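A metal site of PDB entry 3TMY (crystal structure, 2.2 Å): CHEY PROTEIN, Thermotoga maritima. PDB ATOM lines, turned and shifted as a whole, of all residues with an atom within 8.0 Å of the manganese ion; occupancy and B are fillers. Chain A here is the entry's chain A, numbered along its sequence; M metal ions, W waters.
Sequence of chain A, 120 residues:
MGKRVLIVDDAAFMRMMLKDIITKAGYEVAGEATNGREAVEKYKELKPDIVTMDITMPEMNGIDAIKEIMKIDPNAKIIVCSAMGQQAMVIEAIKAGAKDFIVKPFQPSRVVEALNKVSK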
ATOM      1  N   VAL A   8       5.173  18.127 -31.677  1.00  0.00           N
ATOM      2  CA  VAL A   8       3.911  18.616 -31.139  1.00  0.00           C
ATOM      3  C   VAL A   8       4.077  19.039 -29.714  1.00  0.00           C
ATOM      4  O   VAL A   8       4.421  18.216 -28.841  1.00  0.00           O
ATOM      5  CB  VAL A   8       2.923  17.458 -31.176  1.00  0.00           C
ATOM      6  CG1 VAL A   8       1.556  17.790 -30.621  1.00  0.00           C
ATOM      7  CG2 VAL A   8       2.847  16.871 -32.553  1.00  0.00           C
ATOM      8  N   ASP A   9       3.773  20.329 -29.443  1.00  0.00           N
ATOM      9  CA  ASP A   9       3.835  20.908 -28.109  1.00  0.00           C
ATOM     10  C   ASP A   9       3.263  22.291 -28.218  1.00  0.00           C
ATOM     11  O   ASP A   9       3.427  22.938 -29.249  1.00  0.00           O
ATOM     12  CB  ASP A   9       5.320  20.931 -27.601  1.00  0.00           C
ATOM     13  CG  ASP A   9       5.520  21.312 -26.176  1.00  0.00           C
ATOM     14  OD1 ASP A   9       5.096  22.327 -25.717  1.00  0.00           O
ATOM     15  OD2 ASP A   9       6.371  20.539 -25.547  1.00  0.00           O
ATOM     16  N   ASP A  10       2.495  22.652 -27.188  1.00  0.00           N
ATOM     17  CA  ASP A  10       1.768  23.924 -27.102  1.00  0.00           C
ATOM     18  C   ASP A  10       2.736  25.048 -26.725  1.00  0.00           C
ATOM     19  O   ASP A  10       2.407  26.240 -26.835  1.00  0.00           O
ATOM     20  CB  ASP A  10       0.567  23.852 -26.070  1.00  0.00           C
ATOM     21  CG  ASP A  10       0.945  23.156 -24.762  1.00  0.00           C
ATOM     22  OD1 ASP A  10       1.696  22.178 -24.737  1.00  0.00           O
ATOM     23  OD2 ASP A  10       0.446  23.701 -23.649  1.00  0.00           O
ATOM     24  N   ALA A  11       3.905  24.684 -26.223  1.00  0.00           N
ATOM     25  CA  ALA A  11       4.926  25.644 -25.869  1.00  0.00           C
ATOM     26  C   ALA A  11       5.911  25.815 -27.012  1.00  0.00           C
ATOM     27  O   ALA A  11       6.616  24.884 -27.414  1.00  0.00           O
ATOM     28  CB  ALA A  11       5.638  25.342 -24.577  1.00  0.00           C
ATOM     29  N   MET A  14       9.590  25.300 -26.304  1.00  0.00           N
ATOM     30  CA  MET A  14       9.751  23.866 -26.291  1.00  0.00           C
ATOM     31  C   MET A  14       9.798  23.287 -27.661  1.00  0.00           C
ATOM     32  O   MET A  14      10.625  22.424 -27.947  1.00  0.00           O
ATOM     33  CB  MET A  14       8.577  23.229 -25.606  1.00  0.00           C
ATOM     34  CG  MET A  14       9.068  22.348 -24.548  1.00  0.00           C
ATOM     35  SD  MET A  14       9.813  23.267 -23.206  1.00  0.00           S
ATOM     36  CE  MET A  14      11.371  22.379 -23.053  1.00  0.00           C
ATOM     37  N   THR A  34       0.467  22.373 -32.381  1.00  0.00           N
ATOM     38  CA  THR A  34       0.298  23.062 -31.113  1.00  0.00           C
ATOM     39  C   THR A  34      -0.673  22.410 -30.135  1.00  0.00           C
ATOM     40  O   THR A  34      -0.820  22.924 -29.002  1.00  0.00           O
ATOM     41  CB  THR A  34      -0.127  24.534 -31.334  1.00  0.00           C
ATOM     42  OG1 THR A  34      -1.003  24.614 -32.457  1.00  0.00           O
ATOM     43  CG2 THR A  34       1.103  25.391 -31.610  1.00  0.00           C
ATOM     44  N   ASP A  54       3.941  16.012 -26.871  1.00  0.00           N
ATOM     45  CA  ASP A  54       3.756  16.559 -25.525  1.00  0.00           C
ATOM     46  C   ASP A  54       2.482  15.976 -24.785  1.00  0.00           C
ATOM     47  O   ASP A  54       1.483  15.603 -25.399  1.00  0.00           O
ATOM     48  CB  ASP A  54       3.721  18.088 -25.548  1.00  0.00           C
ATOM     49  CG  ASP A  54       3.696  18.613 -24.179  1.00  0.00           C
ATOM     50  OD1 ASP A  54       4.047  17.924 -23.219  1.00  0.00           O
ATOM     51  OD2 ASP A  54       2.955  19.671 -24.089  1.00  0.00           O
ATOM     52  N   ILE A  55       2.488  15.881 -23.463  1.00  0.00           N
ATOM     53  CA  ILE A  55       1.333  15.298 -22.773  1.00  0.00           C
ATOM     54  C   ILE A  55       0.227  16.286 -22.413  1.00  0.00           C
ATOM     55  O   ILE A  55      -0.917  16.096 -22.768  1.00  0.00           O
ATOM     56  CB  ILE A  55       1.723  14.474 -21.560  1.00  0.00           C
ATOM     57  CG1 ILE A  55       2.445  13.203 -21.981  1.00  0.00           C
ATOM     58  CG2 ILE A  55       0.455  14.111 -20.801  1.00  0.00           C
ATOM     59  CD1 ILE A  55       3.162  12.538 -20.804  1.00  0.00           C
ATOM     60  N   THR A  56       0.550  17.362 -21.740  1.00  0.00           N
ATOM     61  CA  THR A  56      -0.438  18.331 -21.389  1.00  0.00           C
ATOM     62  C   THR A  56      -0.499  19.365 -22.447  1.00  0.00           C
ATOM     63  O   THR A  56       0.489  20.030 -22.704  1.00  0.00           O
ATOM     64  CB  THR A  56      -0.113  18.968 -20.048  1.00  0.00           C
ATOM     65  OG1 THR A  56      -0.105  17.959 -19.077  1.00  0.00           O
ATOM     66  CG2 THR A  56      -1.176  19.971 -19.696  1.00  0.00           C
ATOM     67  N   MET A  57      -1.661  19.399 -23.102  1.00  0.00           N
ATOM     68  CA  MET A  57      -2.013  20.284 -24.203  1.00  0.00           C
ATOM     69  C   MET A  57      -3.510  20.519 -24.216  1.00  0.00           C
ATOM     70  O   MET A  57      -4.295  19.727 -23.694  1.00  0.00           O
ATOM     71  CB  MET A  57      -1.605  19.673 -25.569  1.00  0.00           C
ATOM     72  CG  MET A  57      -0.117  19.334 -25.718  1.00  0.00           C
ATOM     73  SD  MET A  57       0.202  19.064 -27.488  1.00  0.00           S
ATOM     74  CE  MET A  57      -0.390  17.376 -27.639  1.00  0.00           C
ATOM     75  N   PRO A  58      -3.859  21.603 -24.895  1.00  0.00           N
ATOM     76  CA  PRO A  58      -5.220  22.044 -25.019  1.00  0.00           C
ATOM     77  C   PRO A  58      -5.933  21.356 -26.151  1.00  0.00           C
ATOM     78  O   PRO A  58      -5.306  20.919 -27.131  1.00  0.00           O
ATOM     79  CB  PRO A  58      -5.137  23.554 -25.309  1.00  0.00           C
ATOM     80  CG  PRO A  58      -3.709  24.008 -25.103  1.00  0.00           C
ATOM     81  CD  PRO A  58      -2.912  22.770 -24.740  1.00  0.00           C
ATOM     82  N   CYS A  81       6.692  13.300 -24.636  1.00  0.00           N
ATOM     83  CA  CYS A  81       7.481  14.233 -23.815  1.00  0.00           C
ATOM     84  C   CYS A  81       6.716  14.571 -22.575  1.00  0.00           C
ATOM     85  O   CYS A  81       5.596  14.992 -22.680  1.00  0.00           O
ATOM     86  CB  CYS A  81       7.752  15.592 -24.525  1.00  0.00           C
ATOM     87  SG  CYS A  81       8.296  15.297 -26.218  1.00  0.00           S
ATOM     88  N   GLN A  86       5.264  13.270 -14.256  1.00  0.00           N
ATOM     89  CA  GLN A  86       4.137  12.981 -15.116  1.00  0.00           C
ATOM     90  C   GLN A  86       4.141  11.470 -15.410  1.00  0.00           C
ATOM     91  O   GLN A  86       3.532  10.995 -16.408  1.00  0.00           O
ATOM     92  CB  GLN A  86       4.053  13.848 -16.399  1.00  0.00           C
ATOM     93  CG  GLN A  86       3.360  15.218 -16.203  1.00  0.00           C
ATOM     94  CD  GLN A  86       3.438  16.117 -17.428  1.00  0.00           C
ATOM     95  OE1 GLN A  86       3.325  17.349 -17.317  1.00  0.00           O
ATOM     96  NE2 GLN A  86       3.651  15.541 -18.614  1.00  0.00           N
ATOM     97  N   LYS A 104      11.360  16.683 -19.992  1.00  0.00           N
ATOM     98  CA  LYS A 104      11.651  18.057 -20.074  1.00  0.00           C
ATOM     99  C   LYS A 104      12.036  18.478 -18.705  1.00  0.00           C
ATOM    100  O   LYS A 104      11.495  17.969 -17.707  1.00  0.00           O
ATOM    101  CB  LYS A 104      10.414  18.781 -20.472  1.00  0.00           C
ATOM    102  CG  LYS A 104      10.082  18.466 -21.895  1.00  0.00           C
ATOM    103  CD  LYS A 104       8.574  18.269 -22.094  1.00  0.00           C
ATOM    104  CE  LYS A 104       7.811  19.587 -22.178  1.00  0.00           C
ATOM    105  NZ  LYS A 104       6.586  19.507 -23.015  1.00  0.00           N
HETATM  106 MN    MN M   1       2.279  21.351 -22.865  1.00  0.00          MN
HETATM  107  O   HOH W   1       4.395  22.581 -23.085  1.00  0.00           O
HETATM  108  O   HOH W   2       1.008  22.490 -21.265  1.00  0.00           O
HETATM  109  O   HOH W   3       2.592  20.294 -21.119  1.00  0.00           O
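The side-chain carboxylate (OD1) of Asp 54 lies within salt-bridge range of the side-chain amino group (NZ) of Lys 104, at 3.0 Å.
The backbone carbonyl oxygen of Val 8 sits at hydrogen-bond distance from the backbone NH of Asp 54 (3.0 Å).
Of the 14 residues printed, 3 come within 4 Å of the manganese ion.
The manganese ion is bound by water W3, OD1 of Asp 10, OD2 of Asp 54, O of Thr 56, water W2 and water W1.
The manganese ion has six donor atoms within binding distance.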
